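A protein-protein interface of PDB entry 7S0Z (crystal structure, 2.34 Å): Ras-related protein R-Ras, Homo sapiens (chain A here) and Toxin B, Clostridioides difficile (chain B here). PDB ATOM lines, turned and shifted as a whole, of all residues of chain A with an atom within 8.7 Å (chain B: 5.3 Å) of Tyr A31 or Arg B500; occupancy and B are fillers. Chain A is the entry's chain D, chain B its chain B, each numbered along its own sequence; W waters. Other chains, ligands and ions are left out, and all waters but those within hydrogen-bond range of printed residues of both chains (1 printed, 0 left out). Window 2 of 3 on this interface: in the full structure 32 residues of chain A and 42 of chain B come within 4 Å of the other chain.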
ATOM      1  N   SER A  21     -12.389 -22.843  21.258  1.00  0.00           N
ATOM      2  CA  SER A  21     -12.897 -23.559  20.057  1.00  0.00           C
ATOM      3  C   SER A  21     -14.159 -22.864  19.544  1.00  0.00           C
ATOM      4  O   SER A  21     -14.269 -22.662  18.321  1.00  0.00           O
ATOM      5  CB  SER A  21     -13.163 -25.013  20.341  1.00  0.00           C
ATOM      6  OG  SER A  21     -11.950 -25.743  20.426  1.00  0.00           O
ATOM      7  N   ALA A  22     -15.076 -22.515  20.441  1.00  0.00           N
ATOM      8  CA  ALA A  22     -16.348 -21.871  20.056  1.00  0.00           C
ATOM      9  C   ALA A  22     -16.050 -20.537  19.367  1.00  0.00           C
ATOM     10  O   ALA A  22     -16.654 -20.281  18.307  1.00  0.00           O
ATOM     11  CB  ALA A  22     -17.238 -21.704  21.257  1.00  0.00           C
ATOM     12  N   LEU A  23     -15.149 -19.726  19.924  1.00  0.00           N
ATOM     13  CA  LEU A  23     -14.771 -18.429  19.302  1.00  0.00           C
ATOM     14  C   LEU A  23     -14.153 -18.694  17.926  1.00  0.00           C
ATOM     15  O   LEU A  23     -14.587 -18.058  16.935  1.00  0.00           O
ATOM     16  CB  LEU A  23     -13.785 -17.668  20.192  1.00  0.00           C
ATOM     17  CG  LEU A  23     -14.353 -16.988  21.438  1.00  0.00           C
ATOM     18  CD1 LEU A  23     -13.217 -16.419  22.265  1.00  0.00           C
ATOM     19  CD2 LEU A  23     -15.350 -15.891  21.094  1.00  0.00           C
ATOM     20  N   THR A  24     -13.175 -19.595  17.867  1.00  0.00           N
ATOM     21  CA  THR A  24     -12.405 -19.865  16.629  1.00  0.00           C
ATOM     22  C   THR A  24     -13.363 -20.332  15.533  1.00  0.00           C
ATOM     23  O   THR A  24     -13.307 -19.785  14.425  1.00  0.00           O
ATOM     24  CB  THR A  24     -11.303 -20.895  16.873  1.00  0.00           C
ATOM     25  OG1 THR A  24     -10.510 -20.450  17.974  1.00  0.00           O
ATOM     26  CG2 THR A  24     -10.435 -21.075  15.649  1.00  0.00           C
ATOM     27  N   ILE A  25     -14.223 -21.293  15.849  1.00  0.00           N
ATOM     28  CA  ILE A  25     -15.179 -21.869  14.862  1.00  0.00           C
ATOM     29  C   ILE A  25     -16.155 -20.781  14.418  1.00  0.00           C
ATOM     30  O   ILE A  25     -16.427 -20.701  13.213  1.00  0.00           O
ATOM     31  CB  ILE A  25     -15.885 -23.101  15.447  1.00  0.00           C
ATOM     32  CG1 ILE A  25     -14.881 -24.245  15.607  1.00  0.00           C
ATOM     33  CG2 ILE A  25     -17.087 -23.494  14.593  1.00  0.00           C
ATOM     34  CD1 ILE A  25     -15.427 -25.467  16.317  1.00  0.00           C
ATOM     35  N   GLN A  26     -16.659 -19.967  15.343  1.00  0.00           N
ATOM     36  CA  GLN A  26     -17.545 -18.833  14.972  1.00  0.00           C
ATOM     37  C   GLN A  26     -16.810 -17.887  14.017  1.00  0.00           C
ATOM     38  O   GLN A  26     -17.426 -17.451  13.030  1.00  0.00           O
ATOM     39  CB  GLN A  26     -18.019 -18.071  16.207  1.00  0.00           C
ATOM     40  CG  GLN A  26     -19.359 -18.551  16.735  1.00  0.00           C
ATOM     41  CD  GLN A  26     -20.536 -18.014  15.956  1.00  0.00           C
ATOM     42  OE1 GLN A  26     -20.494 -17.872  14.738  1.00  0.00           O
ATOM     43  NE2 GLN A  26     -21.615 -17.727  16.663  1.00  0.00           N
ATOM     44  N   PHE A  27     -15.547 -17.574  14.301  1.00  0.00           N
ATOM     45  CA  PHE A  27     -14.736 -16.652  13.467  1.00  0.00           C
ATOM     46  C   PHE A  27     -14.552 -17.240  12.064  1.00  0.00           C
ATOM     47  O   PHE A  27     -14.809 -16.514  11.091  1.00  0.00           O
ATOM     48  CB  PHE A  27     -13.395 -16.355  14.140  1.00  0.00           C
ATOM     49  CG  PHE A  27     -12.482 -15.462  13.339  1.00  0.00           C
ATOM     50  CD1 PHE A  27     -12.914 -14.220  12.900  1.00  0.00           C
ATOM     51  CD2 PHE A  27     -11.187 -15.853  13.037  1.00  0.00           C
ATOM     52  CE1 PHE A  27     -12.075 -13.391  12.171  1.00  0.00           C
ATOM     53  CE2 PHE A  27     -10.347 -15.023  12.311  1.00  0.00           C
ATOM     54  CZ  PHE A  27     -10.793 -13.794  11.877  1.00  0.00           C
ATOM     55  N   ILE A  28     -14.161 -18.511  11.956  1.00  0.00           N
ATOM     56  CA  ILE A  28     -13.858 -19.146  10.637  1.00  0.00           C
ATOM     57  C   ILE A  28     -15.153 -19.376   9.858  1.00  0.00           C
ATOM     58  O   ILE A  28     -15.212 -18.982   8.681  1.00  0.00           O
ATOM     59  CB  ILE A  28     -13.088 -20.469  10.799  1.00  0.00           C
ATOM     60  CG1 ILE A  28     -11.843 -20.287  11.661  1.00  0.00           C
ATOM     61  CG2 ILE A  28     -12.732 -21.041   9.434  1.00  0.00           C
ATOM     62  CD1 ILE A  28     -10.916 -19.232  11.130  1.00  0.00           C
ATOM     63  N   GLN A  29     -16.124 -20.038  10.478  1.00  0.00           N
ATOM     64  CA  GLN A  29     -17.216 -20.733   9.745  1.00  0.00           C
ATOM     65  C   GLN A  29     -18.595 -20.240  10.190  1.00  0.00           C
ATOM     66  O   GLN A  29     -19.584 -20.688   9.588  1.00  0.00           O
ATOM     67  CB  GLN A  29     -17.084 -22.244   9.956  1.00  0.00           C
ATOM     68  CG  GLN A  29     -15.994 -22.881   9.099  1.00  0.00           C
ATOM     69  CD  GLN A  29     -15.201 -23.961   9.798  1.00  0.00           C
ATOM     70  OE1 GLN A  29     -14.088 -24.294   9.390  1.00  0.00           O
ATOM     71  NE2 GLN A  29     -15.761 -24.528  10.857  1.00  0.00           N
ATOM     72  N   SER A  30     -18.670 -19.352  11.180  1.00  0.00           N
ATOM     73  CA  SER A  30     -19.949 -18.775  11.670  1.00  0.00           C
ATOM     74  C   SER A  30     -20.908 -19.892  12.090  1.00  0.00           C
ATOM     75  O   SER A  30     -22.102 -19.807  11.740  1.00  0.00           O
ATOM     76  CB  SER A  30     -20.577 -17.896  10.618  1.00  0.00           C
ATOM     77  OG  SER A  30     -19.711 -16.832  10.264  1.00  0.00           O
ATOM     78  N   TYR A  31     -20.403 -20.901  12.801  1.00  0.00           N
ATOM     79  CA  TYR A  31     -21.234 -21.944  13.455  1.00  0.00           C
ATOM     80  C   TYR A  31     -21.027 -21.891  14.962  1.00  0.00           C
ATOM     81  O   TYR A  31     -19.883 -21.765  15.435  1.00  0.00           O
ATOM     82  CB  TYR A  31     -20.901 -23.355  12.974  1.00  0.00           C
ATOM     83  CG  TYR A  31     -21.330 -23.656  11.566  1.00  0.00           C
ATOM     84  CD1 TYR A  31     -22.654 -23.558  11.162  1.00  0.00           C
ATOM     85  CD2 TYR A  31     -20.393 -24.037  10.627  1.00  0.00           C
ATOM     86  CE1 TYR A  31     -23.031 -23.835   9.857  1.00  0.00           C
ATOM     87  CE2 TYR A  31     -20.750 -24.324   9.323  1.00  0.00           C
ATOM     88  CZ  TYR A  31     -22.074 -24.223   8.934  1.00  0.00           C
ATOM     89  OH  TYR A  31     -22.418 -24.501   7.641  1.00  0.00           O
ATOM     90  N   PHE A  32     -22.135 -21.988  15.680  1.00  0.00           N
ATOM     91  CA  PHE A  32     -22.165 -22.288  17.126  1.00  0.00           C
ATOM     92  C   PHE A  32     -23.344 -23.215  17.376  1.00  0.00           C
ATOM     93  O   PHE A  32     -24.444 -22.962  16.848  1.00  0.00           O
ATOM     94  CB  PHE A  32     -22.286 -21.017  17.966  1.00  0.00           C
ATOM     95  CG  PHE A  32     -22.255 -21.261  19.456  1.00  0.00           C
ATOM     96  CD1 PHE A  32     -23.397 -21.658  20.138  1.00  0.00           C
ATOM     97  CD2 PHE A  32     -21.077 -21.118  20.173  1.00  0.00           C
ATOM     98  CE1 PHE A  32     -23.364 -21.892  21.504  1.00  0.00           C
ATOM     99  CE2 PHE A  32     -21.045 -21.350  21.541  1.00  0.00           C
ATOM    100  CZ  PHE A  32     -22.188 -21.736  22.204  1.00  0.00           C
ATOM    101  N   VAL A  33     -23.099 -24.264  18.150  1.00  0.00           N
ATOM    102  CA  VAL A  33     -24.154 -25.220  18.574  1.00  0.00           C
ATOM    103  C   VAL A  33     -23.870 -25.611  20.018  1.00  0.00           C
ATOM    104  O   VAL A  33     -22.787 -26.174  20.283  1.00  0.00           O
ATOM    105  CB  VAL A  33     -24.219 -26.466  17.676  1.00  0.00           C
ATOM    106  CG1 VAL A  33     -25.420 -27.319  18.055  1.00  0.00           C
ATOM    107  CG2 VAL A  33     -24.248 -26.114  16.196  1.00  0.00           C
ATOM    108  N   SER A  34     -24.809 -25.312  20.911  1.00  0.00           N
ATOM    109  CA  SER A  34     -24.743 -25.773  22.318  1.00  0.00           C
ATOM    110  C   SER A  34     -24.849 -27.296  22.322  1.00  0.00           C
ATOM    111  O   SER A  34     -25.563 -27.844  21.459  1.00  0.00           O
ATOM    112  CB  SER A  34     -25.820 -25.157  23.166  1.00  0.00           C
ATOM    113  OG  SER A  34     -26.107 -23.830  22.748  1.00  0.00           O
ATOM    114  N   TYR A  36     -22.996 -29.684  21.417  1.00  0.00           N
ATOM    115  CA  TYR A  36     -22.537 -30.403  20.198  1.00  0.00           C
ATOM    116  C   TYR A  36     -21.087 -30.028  19.907  1.00  0.00           C
ATOM    117  O   TYR A  36     -20.836 -29.023  19.213  1.00  0.00           O
ATOM    118  CB  TYR A  36     -23.448 -30.112  19.001  1.00  0.00           C
ATOM    119  CG  TYR A  36     -23.051 -30.806  17.717  1.00  0.00           C
ATOM    120  CD1 TYR A  36     -22.985 -32.190  17.640  1.00  0.00           C
ATOM    121  CD2 TYR A  36     -22.755 -30.086  16.566  1.00  0.00           C
ATOM    122  CE1 TYR A  36     -22.629 -32.838  16.466  1.00  0.00           C
ATOM    123  CE2 TYR A  36     -22.403 -30.718  15.383  1.00  0.00           C
ATOM    124  CZ  TYR A  36     -22.336 -32.099  15.333  1.00  0.00           C
ATOM    125  OH  TYR A  36     -21.990 -32.727  14.172  1.00  0.00           O
ATOM    126  N   ILE A  40     -13.879 -32.568  15.452  1.00  0.00           N
ATOM    127  CA  ILE A  40     -13.611 -32.119  14.062  1.00  0.00           C
ATOM    128  C   ILE A  40     -12.127 -31.806  13.928  1.00  0.00           C
ATOM    129  O   ILE A  40     -11.433 -31.676  14.959  1.00  0.00           O
ATOM    130  CB  ILE A  40     -14.464 -30.893  13.712  1.00  0.00           C
ATOM    131  CG1 ILE A  40     -14.251 -29.780  14.742  1.00  0.00           C
ATOM    132  CG2 ILE A  40     -15.925 -31.288  13.572  1.00  0.00           C
ATOM    133  CD1 ILE A  40     -14.651 -28.417  14.274  1.00  0.00           C
ATOM    134  N   ALA A 151     -19.203 -16.021  21.749  1.00  0.00           N
ATOM    135  CA  ALA A 151     -19.224 -16.980  20.624  1.00  0.00           C
ATOM    136  C   ALA A 151     -20.672 -17.413  20.371  1.00  0.00           C
ATOM    137  O   ALA A 151     -21.027 -17.619  19.199  1.00  0.00           O
ATOM    138  CB  ALA A 151     -18.336 -18.161  20.904  1.00  0.00           C
ATOM    139  N   LYS A 152     -21.490 -17.502  21.421  1.00  0.00           N
ATOM    140  CA  LYS A 152     -22.896 -17.973  21.305  1.00  0.00           C
ATOM    141  C   LYS A 152     -23.724 -17.000  20.457  1.00  0.00           C
ATOM    142  O   LYS A 152     -24.495 -17.483  19.603  1.00  0.00           O
ATOM    143  CB  LYS A 152     -23.518 -18.158  22.690  1.00  0.00           C
ATOM    144  CG  LYS A 152     -24.960 -18.654  22.699  1.00  0.00           C
ATOM    145  CD  LYS A 152     -25.238 -19.622  23.833  1.00  0.00           C
ATOM    146  CE  LYS A 152     -26.664 -19.619  24.354  1.00  0.00           C
ATOM    147  NZ  LYS A 152     -27.681 -19.357  23.306  1.00  0.00           N
ATOM    148  N   ARG A 154     -22.338 -14.562  18.599  1.00  0.00           N
ATOM    149  CA  ARG A 154     -21.358 -14.002  17.637  1.00  0.00           C
ATOM    150  C   ARG A 154     -21.256 -12.493  17.863  1.00  0.00           C
ATOM    151  O   ARG A 154     -21.496 -11.713  16.915  1.00  0.00           O
ATOM    152  CB  ARG A 154     -21.736 -14.341  16.196  1.00  0.00           C
ATOM    153  CG  ARG A 154     -20.525 -14.311  15.276  1.00  0.00           C
ATOM    154  CD  ARG A 154     -20.802 -14.780  13.867  1.00  0.00           C
ATOM    155  NE  ARG A 154     -19.566 -15.166  13.194  1.00  0.00           N
ATOM    156  CZ  ARG A 154     -18.742 -14.330  12.570  1.00  0.00           C
ATOM    157  NH1 ARG A 154     -19.016 -13.036  12.519  1.00  0.00           N
ATOM    158  NH2 ARG A 154     -17.647 -14.792  11.990  1.00  0.00           N
ATOM    159  N   VAL A 157     -16.796 -11.223  17.905  1.00  0.00           N
ATOM    160  CA  VAL A 157     -15.893 -12.346  17.521  1.00  0.00           C
ATOM    161  C   VAL A 157     -14.967 -11.870  16.400  1.00  0.00           C
ATOM    162  O   VAL A 157     -13.737 -11.937  16.585  1.00  0.00           O
ATOM    163  CB  VAL A 157     -16.672 -13.607  17.120  1.00  0.00           C
ATOM    164  CG1 VAL A 157     -15.720 -14.711  16.680  1.00  0.00           C
ATOM    165  CG2 VAL A 157     -17.569 -14.070  18.258  1.00  0.00           C
ATOM    166  N   PHE B 378     -18.722 -33.411   7.161  1.00  0.00           N
ATOM    167  CA  PHE B 378     -18.504 -32.065   7.733  1.00  0.00           C
ATOM    168  C   PHE B 378     -19.381 -31.934   8.968  1.00  0.00           C
ATOM    169  O   PHE B 378     -20.543 -32.387   8.948  1.00  0.00           O
ATOM    170  CB  PHE B 378     -18.847 -30.972   6.722  1.00  0.00           C
ATOM    171  CG  PHE B 378     -17.714 -30.575   5.812  1.00  0.00           C
ATOM    172  CD1 PHE B 378     -17.225 -31.453   4.854  1.00  0.00           C
ATOM    173  CD2 PHE B 378     -17.146 -29.315   5.905  1.00  0.00           C
ATOM    174  CE1 PHE B 378     -16.190 -31.076   4.012  1.00  0.00           C
ATOM    175  CE2 PHE B 378     -16.109 -28.940   5.063  1.00  0.00           C
ATOM    176  CZ  PHE B 378     -15.631 -29.820   4.119  1.00  0.00           C
ATOM    177  N   LYS B 380     -20.163 -28.710  11.858  1.00  0.00           N
ATOM    178  CA  LYS B 380     -19.930 -27.264  12.093  1.00  0.00           C
ATOM    179  C   LYS B 380     -18.948 -26.725  11.049  1.00  0.00           C
ATOM    180  O   LYS B 380     -18.115 -25.875  11.408  1.00  0.00           O
ATOM    181  CB  LYS B 380     -19.351 -27.050  13.491  1.00  0.00           C
ATOM    182  CG  LYS B 380     -20.311 -27.323  14.634  1.00  0.00           C
ATOM    183  CD  LYS B 380     -19.563 -27.761  15.865  1.00  0.00           C
ATOM    184  CE  LYS B 380     -19.862 -26.918  17.079  1.00  0.00           C
ATOM    185  NZ  LYS B 380     -18.807 -27.076  18.106  1.00  0.00           N
ATOM    186  N   GLY B 381     -19.025 -27.219   9.813  1.00  0.00           N
ATOM    187  CA  GLY B 381     -18.212 -26.706   8.692  1.00  0.00           C
ATOM    188  C   GLY B 381     -16.754 -27.135   8.723  1.00  0.00           C
ATOM    189  O   GLY B 381     -15.985 -26.589   7.916  1.00  0.00           O
ATOM    190  N   SER B 496     -11.582 -24.293   3.933  1.00  0.00           N
ATOM    191  CA  SER B 496     -12.834 -25.051   3.692  1.00  0.00           C
ATOM    192  C   SER B 496     -13.268 -24.865   2.237  1.00  0.00           C
ATOM    193  O   SER B 496     -13.823 -25.814   1.654  1.00  0.00           O
ATOM    194  CB  SER B 496     -13.910 -24.614   4.630  1.00  0.00           C
ATOM    195  OG  SER B 496     -14.011 -23.199   4.641  1.00  0.00           O
ATOM    196  N   SER B 497     -13.020 -23.681   1.678  1.00  0.00           N
ATOM    197  CA  SER B 497     -13.258 -23.371   0.245  1.00  0.00           C
ATOM    198  C   SER B 497     -12.694 -24.493  -0.641  1.00  0.00           C
ATOM    199  O   SER B 497     -13.302 -24.773  -1.692  1.00  0.00           O
ATOM    200  CB  SER B 497     -12.687 -22.022  -0.100  1.00  0.00           C
ATOM    201  OG  SER B 497     -12.237 -21.976  -1.442  1.00  0.00           O
ATOM    202  N   GLU B 498     -11.589 -25.123  -0.234  1.00  0.00           N
ATOM    203  CA  GLU B 498     -11.007 -26.275  -0.978  1.00  0.00           C
ATOM    204  C   GLU B 498     -11.613 -27.581  -0.457  1.00  0.00           C
ATOM    205  O   GLU B 498     -11.910 -28.453  -1.294  1.00  0.00           O
ATOM    206  CB  GLU B 498      -9.483 -26.291  -0.863  1.00  0.00           C
ATOM    207  CG  GLU B 498      -8.890 -24.904  -0.744  1.00  0.00           C
ATOM    208  CD  GLU B 498      -7.377 -24.835  -0.762  1.00  0.00           C
ATOM    209  OE1 GLU B 498      -6.769 -25.347  -1.726  1.00  0.00           O
ATOM    210  OE2 GLU B 498      -6.815 -24.269   0.196  1.00  0.00           O
ATOM    211  N   LEU B 499     -11.797 -27.713   0.858  1.00  0.00           N
ATOM    212  CA  LEU B 499     -12.227 -28.998   1.467  1.00  0.00           C
ATOM    213  C   LEU B 499     -13.670 -29.315   1.077  1.00  0.00           C
ATOM    214  O   LEU B 499     -13.997 -30.514   1.023  1.00  0.00           O
ATOM    215  CB  LEU B 499     -12.055 -28.949   2.987  1.00  0.00           C
ATOM    216  CG  LEU B 499     -10.608 -28.783   3.448  1.00  0.00           C
ATOM    217  CD1 LEU B 499     -10.517 -28.328   4.897  1.00  0.00           C
ATOM    218  CD2 LEU B 499      -9.825 -30.065   3.242  1.00  0.00           C
ATOM    219  N   ARG B 500     -14.494 -28.308   0.780  1.00  0.00           N
ATOM    220  CA  ARG B 500     -15.921 -28.558   0.445  1.00  0.00           C
ATOM    221  C   ARG B 500     -16.036 -29.379  -0.842  1.00  0.00           C
ATOM    222  O   ARG B 500     -17.134 -29.904  -1.101  1.00  0.00           O
ATOM    223  CB  ARG B 500     -16.704 -27.256   0.281  1.00  0.00           C
ATOM    224  CG  ARG B 500     -17.032 -26.559   1.591  1.00  0.00           C
ATOM    225  CD  ARG B 500     -18.000 -27.347   2.452  1.00  0.00           C
ATOM    226  NE  ARG B 500     -18.222 -26.692   3.738  1.00  0.00           N
ATOM    227  CZ  ARG B 500     -19.341 -26.768   4.460  1.00  0.00           C
ATOM    228  NH1 ARG B 500     -20.376 -27.472   4.032  1.00  0.00           N
ATOM    229  NH2 ARG B 500     -19.426 -26.123   5.610  1.00  0.00           N
ATOM    230  N   ASN B 501     -14.960 -29.488  -1.617  1.00  0.00           N
ATOM    231  CA  ASN B 501     -14.955 -30.284  -2.870  1.00  0.00           C
ATOM    232  C   ASN B 501     -14.985 -31.776  -2.542  1.00  0.00           C
ATOM    233  O   ASN B 501     -15.265 -32.566  -3.456  1.00  0.00           O
ATOM    234  CB  ASN B 501     -13.742 -29.962  -3.740  1.00  0.00           C
ATOM    235  CG  ASN B 501     -13.895 -28.651  -4.481  1.00  0.00           C
ATOM    236  OD1 ASN B 501     -14.892 -28.433  -5.165  1.00  0.00           O
ATOM    237  ND2 ASN B 501     -12.915 -27.771  -4.357  1.00  0.00           N
ATOM    238  N   PHE B 502     -14.710 -32.147  -1.293  1.00  0.00           N
ATOM    239  CA  PHE B 502     -14.581 -33.566  -0.887  1.00  0.00           C
ATOM    240  C   PHE B 502     -15.654 -33.918   0.141  1.00  0.00           C
ATOM    241  O   PHE B 502     -15.449 -34.867   0.915  1.00  0.00           O
ATOM    242  CB  PHE B 502     -13.178 -33.823  -0.336  1.00  0.00           C
ATOM    243  CG  PHE B 502     -12.066 -33.463  -1.291  1.00  0.00           C
ATOM    244  CD1 PHE B 502     -11.617 -34.376  -2.234  1.00  0.00           C
ATOM    245  CD2 PHE B 502     -11.479 -32.209  -1.260  1.00  0.00           C
ATOM    246  CE1 PHE B 502     -10.598 -34.049  -3.116  1.00  0.00           C
ATOM    247  CE2 PHE B 502     -10.461 -31.879  -2.144  1.00  0.00           C
ATOM    248  CZ  PHE B 502     -10.020 -32.799  -3.070  1.00  0.00           C
ATOM    249  N   GLU B 503     -16.763 -33.182   0.165  1.00  0.00           N
ATOM    250  CA  GLU B 503     -17.741 -33.340   1.265  1.00  0.00           C
ATOM    251  C   GLU B 503     -18.608 -34.570   1.008  1.00  0.00           C
ATOM    252  O   GLU B 503     -19.194 -34.679  -0.082  1.00  0.00           O
ATOM    253  CB  GLU B 503     -18.613 -32.104   1.444  1.00  0.00           C
ATOM    254  CG  GLU B 503     -19.802 -32.357   2.352  1.00  0.00           C
ATOM    255  CD  GLU B 503     -20.443 -31.089   2.887  1.00  0.00           C
ATOM    256  OE1 GLU B 503     -21.375 -31.186   3.720  1.00  0.00           O
ATOM    257  OE2 GLU B 503     -20.011 -30.003   2.467  1.00  0.00           O
HETATM  258  O   HOH W   1     -19.881 -24.241  18.692  1.00  0.00           O
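Lys B380 touches Tyr A31.
Tyr A31 touches Gly B381.
Arg B500 touches Tyr A31 (NH2 to OH, 3.96 Å).
Tyr A31 touches just these residues of chain B: Lys B380 (3.0 Å), Gly B381 (3.4 Å) and Arg B500 (3.96 Å).
Of chain A, only Tyr A31 (3.96 Å) comes within 4 Å of Arg B500.
Of chain A, only Gln A29 (3.3 Å) and Tyr A31 (3.4 Å) come within 4 Å of Gly B381.
Of the printed residues of chain A, Lys B380 touches Gln A29, Tyr A31 and Tyr A36.
Printed residues of chain B within 4 Å of Gln A29: Lys B380 (2.8 Å) and Gly B381 (3.3 Å).
Ser B496 touches none of the printed residues of chain A.
Val A157 touches none of the printed residues of chain B.
The nearest printed residue of chain B that does not touch Tyr A31 is Phe B378 (7.0 Å).
The nearest residue of chain A that does not touch Arg B500 is Gln A29 (5.9 Å).
Printed residues of chain B that touch a printed residue of chain A: Lys B380, Gly B381 and Arg B500.
Hydrophobic or aromatic side chains of chain A within 4 Å of the printed part of chain B: Tyr A31.
Among the printed residues, no Asp or Glu carboxylate lies within 4 Å of a Lys or Arg side-chain nitrogen of the other chain.
Water W1 lies within hydrogen-bond range of NZ of Lys B380 (3.1 Å) and N of Val A33 (3.3 Å).
NH1 of Arg B500 is in salt-bridge range of OE2 of Glu B503 (3.0 Å).
The backbone carbonyl oxygen of Lys B380 is in hydrogen-bond range of the side-chain amide nitrogen of Gln A29 (2.8 Å).
The backbone carbonyl oxygen (O) of Tyr A36 is in hydrogen-bond range of the side-chain amino group (NZ) of Lys B380.
OE1 of Gln A29 lies close to O of Gly B381, at 3.3 Å.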
